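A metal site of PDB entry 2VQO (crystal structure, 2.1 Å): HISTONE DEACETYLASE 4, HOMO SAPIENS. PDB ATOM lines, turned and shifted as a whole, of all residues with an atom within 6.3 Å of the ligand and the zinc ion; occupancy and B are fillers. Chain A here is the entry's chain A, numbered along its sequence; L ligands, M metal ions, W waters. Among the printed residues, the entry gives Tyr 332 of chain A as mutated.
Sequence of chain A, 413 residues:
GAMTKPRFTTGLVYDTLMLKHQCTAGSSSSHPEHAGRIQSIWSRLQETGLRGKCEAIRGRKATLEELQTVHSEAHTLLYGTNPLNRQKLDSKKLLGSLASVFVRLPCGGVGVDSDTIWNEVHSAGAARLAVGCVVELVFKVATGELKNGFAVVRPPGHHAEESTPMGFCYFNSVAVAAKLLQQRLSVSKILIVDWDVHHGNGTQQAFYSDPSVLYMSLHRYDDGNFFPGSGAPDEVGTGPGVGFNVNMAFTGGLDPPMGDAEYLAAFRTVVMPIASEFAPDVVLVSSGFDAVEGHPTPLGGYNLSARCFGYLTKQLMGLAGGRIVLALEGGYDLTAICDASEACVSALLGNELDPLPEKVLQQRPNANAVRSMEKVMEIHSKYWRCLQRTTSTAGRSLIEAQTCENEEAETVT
Of the 23 residues printed, 3 come within 4 Å of the zinc ion. Along chain A the residues within 4 Å of the zinc ion span positions 196 to 290.
The zinc ion is bound by OD2 of Asp 196, 1.9 Å away. The zinc ion is bound by OD2 of Asp 290. A ring nitrogen (ND1) of His 198 is bound to the zinc ion, 2.1 Å away. The zinc ion is bound by O2 of the ligand, at 2.2 Å. The zinc ion is bound by O3 of the ligand (2.3 Å).
A ring nitrogen (NE2) of His 158 sits close to an oxygen (O2) of the ligand. A ring nitrogen (NE2) of His 159 sits close to an oxygen (O2) of the ligand (3.0 Å).
Water W2 lies within hydrogen-bond range of the backbone carbonyl oxygen (O) of Pro 298 (2.7 Å), an oxygen (O1) of the ligand (2.7 Å) and a ring nitrogen (NE2) of His 198 (3.0 Å).
O of Glu 329 is in hydrogen-bond range of NH1 of Arg 37 (3.3 Å). OE1 of Glu 329 is in hydrogen-bond range of N of Gly 157 (2.8 Å). The backbone NH (N) of His 158 lies within hydrogen-bond range of the side-chain carboxylate (OE1) of Glu 329, at 3.4 Å. The side-chain sulfur (SG) of Cys 169 is in hydrogen-bond range of the backbone NH (N) of Gly 157, at 3.6 Å. The backbone carbonyl oxygen of Leu 299 lies within hydrogen-bond range of the side-chain hydroxyl of Tyr 332, 3.0 Å away. NE2 of His 159 is in hydrogen-bond range of NE2 of His 158 (3.3 Å). The backbone carbonyl oxygen (O) of Pro 156 sits at hydrogen-bond distance from the side-chain sulfur (SG) of Cys 169 (3.3 Å). The backbone carbonyl oxygen (O) of Gly 167 lies within hydrogen-bond range of the side-chain sulfur (SG) of Cys 169, at 3.3 Å.
The backbone carbonyl oxygen (O) of Gly 167 sits close to a fluorine (F3) of the ligand (3.1 Å). N of Gly 330 sits close to F2 of the ligand (3.1 Å). Pro 156 touches the ligand (CG to F2, 3.5 Å). CD1 of Phe 168 touches C16 of the ligand, at 3.5 Å. Cys 169 touches the ligand (SG to F3, 3.9 Å). Phe 227 touches the ligand. Leu 299 touches the ligand (CD2 to C11, 3.7 Å). Glu 329 touches the ligand (C to F2, 3.6 Å). Of the 23 residues printed, 13 come within 4 Å of the ligand.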
ATOM      1  N   ARG A  37     -14.707 -18.415 -30.363  1.00  0.00           N
ATOM      2  CA  ARG A  37     -15.861 -18.949 -31.113  1.00  0.00           C
ATOM      3  C   ARG A  37     -15.575 -19.214 -32.593  1.00  0.00           C
ATOM      4  O   ARG A  37     -15.761 -20.335 -33.073  1.00  0.00           O
ATOM      5  CB  ARG A  37     -17.071 -18.005 -30.990  1.00  0.00           C
ATOM      6  CG  ARG A  37     -17.596 -17.830 -29.574  1.00  0.00           C
ATOM      7  CD  ARG A  37     -18.911 -17.054 -29.544  1.00  0.00           C
ATOM      8  NE  ARG A  37     -18.824 -15.828 -30.335  1.00  0.00           N
ATOM      9  CZ  ARG A  37     -19.568 -15.517 -31.406  1.00  0.00           C
ATOM     10  NH1 ARG A  37     -20.534 -16.320 -31.837  1.00  0.00           N
ATOM     11  NH2 ARG A  37     -19.355 -14.366 -32.030  1.00  0.00           N
ATOM     12  N   PRO A 156     -20.889 -10.029 -33.786  1.00  0.00           N
ATOM     13  CA  PRO A 156     -22.177 -10.059 -34.477  1.00  0.00           C
ATOM     14  C   PRO A 156     -22.684  -8.646 -34.834  1.00  0.00           C
ATOM     15  O   PRO A 156     -22.093  -7.646 -34.404  1.00  0.00           O
ATOM     16  CB  PRO A 156     -23.103 -10.747 -33.458  1.00  0.00           C
ATOM     17  CG  PRO A 156     -22.487 -10.470 -32.158  1.00  0.00           C
ATOM     18  CD  PRO A 156     -21.019 -10.462 -32.381  1.00  0.00           C
ATOM     19  N   GLY A 157     -23.767  -8.561 -35.609  1.00  0.00           N
ATOM     20  CA  GLY A 157     -24.214  -7.282 -36.141  1.00  0.00           C
ATOM     21  C   GLY A 157     -25.662  -6.862 -35.932  1.00  0.00           C
ATOM     22  O   GLY A 157     -25.978  -5.673 -36.038  1.00  0.00           O
ATOM     23  N   HIS A 158     -26.542  -7.812 -35.639  1.00  0.00           N
ATOM     24  CA  HIS A 158     -27.989  -7.565 -35.776  1.00  0.00           C
ATOM     25  C   HIS A 158     -28.606  -6.654 -34.711  1.00  0.00           C
ATOM     26  O   HIS A 158     -29.730  -6.183 -34.900  1.00  0.00           O
ATOM     27  CB  HIS A 158     -28.770  -8.871 -35.943  1.00  0.00           C
ATOM     28  CG  HIS A 158     -28.885  -9.702 -34.701  1.00  0.00           C
ATOM     29  ND1 HIS A 158     -29.959 -10.533 -34.462  1.00  0.00           N
ATOM     30  CD2 HIS A 158     -28.070  -9.835 -33.626  1.00  0.00           C
ATOM     31  CE1 HIS A 158     -29.797 -11.136 -33.300  1.00  0.00           C
ATOM     32  NE2 HIS A 158     -28.657 -10.731 -32.774  1.00  0.00           N
ATOM     33  N   HIS A 159     -27.894  -6.365 -33.632  1.00  0.00           N
ATOM     34  CA  HIS A 159     -28.385  -5.404 -32.629  1.00  0.00           C
ATOM     35  C   HIS A 159     -27.989  -3.955 -32.934  1.00  0.00           C
ATOM     36  O   HIS A 159     -28.574  -3.039 -32.377  1.00  0.00           O
ATOM     37  CB  HIS A 159     -27.933  -5.763 -31.212  1.00  0.00           C
ATOM     38  CG  HIS A 159     -28.489  -7.054 -30.713  1.00  0.00           C
ATOM     39  ND1 HIS A 159     -29.836  -7.331 -30.688  1.00  0.00           N
ATOM     40  CD2 HIS A 159     -27.867  -8.147 -30.210  1.00  0.00           C
ATOM     41  CE1 HIS A 159     -30.028  -8.535 -30.194  1.00  0.00           C
ATOM     42  NE2 HIS A 159     -28.850  -9.063 -29.897  1.00  0.00           N
ATOM     43  N   MET A 166     -24.789  -1.710 -29.724  1.00  0.00           N
ATOM     44  CA  MET A 166     -25.361  -2.394 -28.567  1.00  0.00           C
ATOM     45  C   MET A 166     -25.293  -3.908 -28.746  1.00  0.00           C
ATOM     46  O   MET A 166     -25.108  -4.395 -29.849  1.00  0.00           O
ATOM     47  CB  MET A 166     -26.815  -1.956 -28.336  1.00  0.00           C
ATOM     48  CG  MET A 166     -27.702  -2.007 -29.559  1.00  0.00           C
ATOM     49  SD  MET A 166     -29.437  -1.617 -29.206  1.00  0.00           S
ATOM     50  CE  MET A 166     -29.886  -2.991 -28.158  1.00  0.00           C
ATOM     51  N   GLY A 167     -25.448  -4.621 -27.640  1.00  0.00           N
ATOM     52  CA  GLY A 167     -25.419  -6.091 -27.641  1.00  0.00           C
ATOM     53  C   GLY A 167     -24.222  -6.668 -28.367  1.00  0.00           C
ATOM     54  O   GLY A 167     -24.366  -7.592 -29.176  1.00  0.00           O
ATOM     55  N   PHE A 168     -23.038  -6.120 -28.103  1.00  0.00           N
ATOM     56  CA  PHE A 168     -21.774  -6.578 -28.717  1.00  0.00           C
ATOM     57  C   PHE A 168     -21.655  -6.232 -30.207  1.00  0.00           C
ATOM     58  O   PHE A 168     -20.681  -6.630 -30.846  1.00  0.00           O
ATOM     59  CB  PHE A 168     -21.580  -8.096 -28.532  1.00  0.00           C
ATOM     60  CG  PHE A 168     -21.681  -8.562 -27.110  1.00  0.00           C
ATOM     61  CD1 PHE A 168     -22.752  -9.322 -26.683  1.00  0.00           C
ATOM     62  CD2 PHE A 168     -20.683  -8.255 -26.189  1.00  0.00           C
ATOM     63  CE1 PHE A 168     -22.850  -9.762 -25.365  1.00  0.00           C
ATOM     64  CE2 PHE A 168     -20.773  -8.681 -24.876  1.00  0.00           C
ATOM     65  CZ  PHE A 168     -21.861  -9.436 -24.466  1.00  0.00           C
ATOM     66  N   CYS A 169     -22.615  -5.474 -30.738  1.00  0.00           N
ATOM     67  CA  CYS A 169     -22.665  -5.163 -32.159  1.00  0.00           C
ATOM     68  C   CYS A 169     -22.262  -3.712 -32.428  1.00  0.00           C
ATOM     69  O   CYS A 169     -22.756  -2.806 -31.784  1.00  0.00           O
ATOM     70  CB  CYS A 169     -24.064  -5.443 -32.731  1.00  0.00           C
ATOM     71  SG  CYS A 169     -24.672  -7.134 -32.476  1.00  0.00           S
ATOM     72  N   ASP A 196     -31.168 -16.244 -34.626  1.00  0.00           N
ATOM     73  CA  ASP A 196     -30.573 -15.975 -33.325  1.00  0.00           C
ATOM     74  C   ASP A 196     -31.723 -15.913 -32.303  1.00  0.00           C
ATOM     75  O   ASP A 196     -32.827 -15.484 -32.655  1.00  0.00           O
ATOM     76  CB  ASP A 196     -29.818 -14.640 -33.380  1.00  0.00           C
ATOM     77  CG  ASP A 196     -28.877 -14.426 -32.204  1.00  0.00           C
ATOM     78  OD1 ASP A 196     -27.660 -14.571 -32.388  1.00  0.00           O
ATOM     79  OD2 ASP A 196     -29.341 -14.112 -31.088  1.00  0.00           O
ATOM     80  N   VAL A 197     -31.491 -16.330 -31.069  1.00  0.00           N
ATOM     81  CA  VAL A 197     -32.579 -16.383 -30.088  1.00  0.00           C
ATOM     82  C   VAL A 197     -33.088 -14.994 -29.656  1.00  0.00           C
ATOM     83  O   VAL A 197     -34.145 -14.884 -29.057  1.00  0.00           O
ATOM     84  CB  VAL A 197     -32.213 -17.252 -28.850  1.00  0.00           C
ATOM     85  CG1 VAL A 197     -31.463 -16.423 -27.790  1.00  0.00           C
ATOM     86  CG2 VAL A 197     -33.465 -17.915 -28.258  1.00  0.00           C
ATOM     87  N   HIS A 198     -32.329 -13.929 -29.954  1.00  0.00           N
ATOM     88  CA  HIS A 198     -32.718 -12.555 -29.620  1.00  0.00           C
ATOM     89  C   HIS A 198     -33.237 -11.810 -30.852  1.00  0.00           C
ATOM     90  O   HIS A 198     -32.800 -12.081 -31.971  1.00  0.00           O
ATOM     91  CB  HIS A 198     -31.522 -11.819 -29.002  1.00  0.00           C
ATOM     92  CG  HIS A 198     -30.952 -12.512 -27.796  1.00  0.00           C
ATOM     93  ND1 HIS A 198     -29.905 -13.402 -27.885  1.00  0.00           N
ATOM     94  CD2 HIS A 198     -31.303 -12.470 -26.499  1.00  0.00           C
ATOM     95  CE1 HIS A 198     -29.624 -13.874 -26.686  1.00  0.00           C
ATOM     96  NE2 HIS A 198     -30.469 -13.325 -25.817  1.00  0.00           N
ATOM     97  N   PHE A 226     -37.508  -9.883 -22.497  1.00  0.00           N
ATOM     98  CA  PHE A 226     -36.280 -10.575 -22.916  1.00  0.00           C
ATOM     99  C   PHE A 226     -35.471  -9.645 -23.828  1.00  0.00           C
ATOM    100  O   PHE A 226     -36.040  -8.910 -24.635  1.00  0.00           O
ATOM    101  CB  PHE A 226     -36.631 -11.881 -23.645  1.00  0.00           C
ATOM    102  CG  PHE A 226     -35.482 -12.849 -23.742  1.00  0.00           C
ATOM    103  CD1 PHE A 226     -34.996 -13.476 -22.610  1.00  0.00           C
ATOM    104  CD2 PHE A 226     -34.897 -13.135 -24.969  1.00  0.00           C
ATOM    105  CE1 PHE A 226     -33.927 -14.368 -22.692  1.00  0.00           C
ATOM    106  CE2 PHE A 226     -33.834 -14.029 -25.064  1.00  0.00           C
ATOM    107  CZ  PHE A 226     -33.355 -14.648 -23.923  1.00  0.00           C
ATOM    108  N   PHE A 227     -34.147  -9.662 -23.687  1.00  0.00           N
ATOM    109  CA  PHE A 227     -33.277  -8.746 -24.414  1.00  0.00           C
ATOM    110  C   PHE A 227     -33.390  -8.929 -25.926  1.00  0.00           C
ATOM    111  O   PHE A 227     -33.405 -10.070 -26.408  1.00  0.00           O
ATOM    112  CB  PHE A 227     -31.812  -8.952 -23.969  1.00  0.00           C
ATOM    113  CG  PHE A 227     -30.822  -8.086 -24.713  1.00  0.00           C
ATOM    114  CD1 PHE A 227     -30.449  -6.850 -24.206  1.00  0.00           C
ATOM    115  CD2 PHE A 227     -30.238  -8.524 -25.891  1.00  0.00           C
ATOM    116  CE1 PHE A 227     -29.520  -6.064 -24.879  1.00  0.00           C
ATOM    117  CE2 PHE A 227     -29.306  -7.735 -26.574  1.00  0.00           C
ATOM    118  CZ  PHE A 227     -28.944  -6.504 -26.061  1.00  0.00           C
ATOM    119  N   PRO A 228     -33.440  -7.821 -26.704  1.00  0.00           N
ATOM    120  CA  PRO A 228     -33.363  -6.408 -26.302  1.00  0.00           C
ATOM    121  C   PRO A 228     -34.726  -5.744 -25.973  1.00  0.00           C
ATOM    122  O   PRO A 228     -34.757  -4.540 -25.748  1.00  0.00           O
ATOM    123  CB  PRO A 228     -32.739  -5.745 -27.529  1.00  0.00           C
ATOM    124  CG  PRO A 228     -33.211  -6.551 -28.661  1.00  0.00           C
ATOM    125  CD  PRO A 228     -33.542  -7.949 -28.159  1.00  0.00           C
ATOM    126  N   GLY A 288     -27.560 -16.991 -35.740  1.00  0.00           N
ATOM    127  CA  GLY A 288     -27.096 -17.140 -34.369  1.00  0.00           C
ATOM    128  C   GLY A 288     -27.555 -18.491 -33.853  1.00  0.00           C
ATOM    129  O   GLY A 288     -28.623 -18.959 -34.232  1.00  0.00           O
ATOM    130  N   ASP A 290     -27.611 -19.384 -30.370  1.00  0.00           N
ATOM    131  CA  ASP A 290     -27.853 -19.347 -28.924  1.00  0.00           C
ATOM    132  C   ASP A 290     -29.162 -20.017 -28.508  1.00  0.00           C
ATOM    133  O   ASP A 290     -29.404 -20.198 -27.318  1.00  0.00           O
ATOM    134  CB  ASP A 290     -27.723 -17.929 -28.337  1.00  0.00           C
ATOM    135  CG  ASP A 290     -28.367 -16.856 -29.211  1.00  0.00           C
ATOM    136  OD1 ASP A 290     -29.090 -17.195 -30.172  1.00  0.00           O
ATOM    137  OD2 ASP A 290     -28.148 -15.664 -28.912  1.00  0.00           O
ATOM    138  N   PRO A 298     -30.945 -16.942 -19.015  1.00  0.00           N
ATOM    139  CA  PRO A 298     -30.984 -15.559 -19.533  1.00  0.00           C
ATOM    140  C   PRO A 298     -30.248 -15.375 -20.867  1.00  0.00           C
ATOM    141  O   PRO A 298     -30.718 -14.621 -21.730  1.00  0.00           O
ATOM    142  CB  PRO A 298     -30.321 -14.743 -18.422  1.00  0.00           C
ATOM    143  CG  PRO A 298     -29.529 -15.714 -17.603  1.00  0.00           C
ATOM    144  CD  PRO A 298     -29.935 -17.128 -17.970  1.00  0.00           C
ATOM    145  N   LEU A 299     -29.114 -16.035 -21.056  1.00  0.00           N
ATOM    146  CA  LEU A 299     -28.346 -15.917 -22.303  1.00  0.00           C
ATOM    147  C   LEU A 299     -28.629 -17.117 -23.193  1.00  0.00           C
ATOM    148  O   LEU A 299     -27.707 -17.787 -23.672  1.00  0.00           O
ATOM    149  CB  LEU A 299     -26.858 -15.788 -22.006  1.00  0.00           C
ATOM    150  CG  LEU A 299     -26.438 -14.509 -21.277  1.00  0.00           C
ATOM    151  CD1 LEU A 299     -25.040 -14.670 -20.698  1.00  0.00           C
ATOM    152  CD2 LEU A 299     -26.506 -13.318 -22.211  1.00  0.00           C
ATOM    153  N   GLU A 329     -24.094 -14.963 -36.022  1.00  0.00           N
ATOM    154  CA  GLU A 329     -24.441 -13.924 -35.068  1.00  0.00           C
ATOM    155  C   GLU A 329     -24.052 -14.392 -33.652  1.00  0.00           C
ATOM    156  O   GLU A 329     -22.874 -14.460 -33.327  1.00  0.00           O
ATOM    157  CB  GLU A 329     -25.922 -13.572 -35.167  1.00  0.00           C
ATOM    158  CG  GLU A 329     -26.345 -12.980 -36.509  1.00  0.00           C
ATOM    159  CD  GLU A 329     -25.937 -11.518 -36.698  1.00  0.00           C
ATOM    160  OE1 GLU A 329     -25.299 -10.931 -35.801  1.00  0.00           O
ATOM    161  OE2 GLU A 329     -26.262 -10.959 -37.768  1.00  0.00           O
ATOM    162  N   GLY A 330     -25.042 -14.735 -32.826  1.00  0.00           N
ATOM    163  CA  GLY A 330     -24.797 -15.162 -31.458  1.00  0.00           C
ATOM    164  C   GLY A 330     -24.643 -16.652 -31.284  1.00  0.00           C
ATOM    165  O   GLY A 330     -24.416 -17.395 -32.243  1.00  0.00           O
ATOM    166  N   GLY A 331     -24.788 -17.097 -30.039  1.00  0.00           N
ATOM    167  CA  GLY A 331     -24.373 -18.439 -29.640  1.00  0.00           C
ATOM    168  C   GLY A 331     -22.948 -18.340 -29.155  1.00  0.00           C
ATOM    169  O   GLY A 331     -22.162 -17.559 -29.689  1.00  0.00           O
ATOM    170  N   TYR A 332     -22.614 -19.098 -28.117  1.00  0.00           N
ATOM    171  CA  TYR A 332     -21.285 -19.009 -27.488  1.00  0.00           C
ATOM    172  C   TYR A 332     -20.747 -20.319 -26.904  1.00  0.00           C
ATOM    173  O   TYR A 332     -19.532 -20.454 -26.706  1.00  0.00           O
ATOM    174  CB  TYR A 332     -21.282 -17.911 -26.409  1.00  0.00           C
ATOM    175  CG  TYR A 332     -22.320 -18.119 -25.337  1.00  0.00           C
ATOM    176  CD1 TYR A 332     -23.545 -17.465 -25.403  1.00  0.00           C
ATOM    177  CD2 TYR A 332     -22.077 -18.956 -24.262  1.00  0.00           C
ATOM    178  CE1 TYR A 332     -24.501 -17.649 -24.426  1.00  0.00           C
ATOM    179  CE2 TYR A 332     -23.026 -19.159 -23.286  1.00  0.00           C
ATOM    180  CZ  TYR A 332     -24.236 -18.499 -23.365  1.00  0.00           C
ATOM    181  OH  TYR A 332     -25.182 -18.700 -22.398  1.00  0.00           O
HETATM  182  C1  LIG L   1     -25.091  -9.629 -17.163  1.00  0.00           C
HETATM  183  C2  LIG L   1     -25.444 -10.133 -15.922  1.00  0.00           C
HETATM  184  C3  LIG L   1     -26.225 -11.286 -15.833  1.00  0.00           C
HETATM  185  C4  LIG L   1     -26.653 -11.924 -16.994  1.00  0.00           C
HETATM  186  C5  LIG L   1     -26.300 -11.419 -18.235  1.00  0.00           C
HETATM  187  C6  LIG L   1     -25.503 -10.271 -18.329  1.00  0.00           C
HETATM  188  C7  LIG L   1     -25.164  -9.707 -19.565  1.00  0.00           C
HETATM  189  C8  LIG L   1     -24.033  -9.150 -19.983  1.00  0.00           C
HETATM  190  N1  LIG L   1     -24.201  -8.718 -21.244  1.00  0.00           N
HETATM  191  C9  LIG L   1     -25.438  -8.982 -21.651  1.00  0.00           C
HETATM  192  C10 LIG L   1     -26.118  -8.671 -23.013  1.00  0.00           C
HETATM  193  N2  LIG L   1     -26.091  -9.608 -20.592  1.00  0.00           N
HETATM  194  C11 LIG L   1     -27.491 -10.063 -20.663  1.00  0.00           C
HETATM  195  C12 LIG L   1     -28.191  -9.422 -21.820  1.00  0.00           C
HETATM  196  N3  LIG L   1     -27.356  -9.461 -23.036  1.00  0.00           N
HETATM  197  C13 LIG L   1     -27.752 -10.262 -24.030  1.00  0.00           C
HETATM  198  O1  LIG L   1     -28.819 -10.842 -23.862  1.00  0.00           O
HETATM  199  C14 LIG L   1     -27.131 -10.422 -25.416  1.00  0.00           C
HETATM  200  S1  LIG L   1     -27.387 -11.761 -26.353  1.00  0.00           S
HETATM  201  C15 LIG L   1     -26.454  -9.517 -26.144  1.00  0.00           C
HETATM  202  C16 LIG L   1     -26.132  -9.947 -27.390  1.00  0.00           C
HETATM  203  C17 LIG L   1     -26.569 -11.192 -27.673  1.00  0.00           C
HETATM  204  C18 LIG L   1     -26.441 -11.985 -28.984  1.00  0.00           C
HETATM  205  C19 LIG L   1     -25.305 -11.498 -29.891  1.00  0.00           C
HETATM  206  F1  LIG L   1     -24.167 -11.547 -29.240  1.00  0.00           F
HETATM  207  F2  LIG L   1     -25.247 -12.282 -30.955  1.00  0.00           F
HETATM  208  F3  LIG L   1     -25.556 -10.242 -30.297  1.00  0.00           F
HETATM  209  O2  LIG L   1     -27.678 -11.810 -29.726  1.00  0.00           O
HETATM  210  O3  LIG L   1     -26.360 -13.398 -28.737  1.00  0.00           O
HETATM  211 ZN    ZN M   1     -28.524 -13.821 -29.425  1.00  0.00          ZN
HETATM  212  O   HOH W   1     -23.382  -6.319 -22.008  1.00  0.00           O
HETATM  213  O   HOH W   2     -30.949 -12.303 -23.004  1.00  0.00           O
HETATM  214  O   HOH W   3     -24.581 -14.867 -27.918  1.00  0.00           O
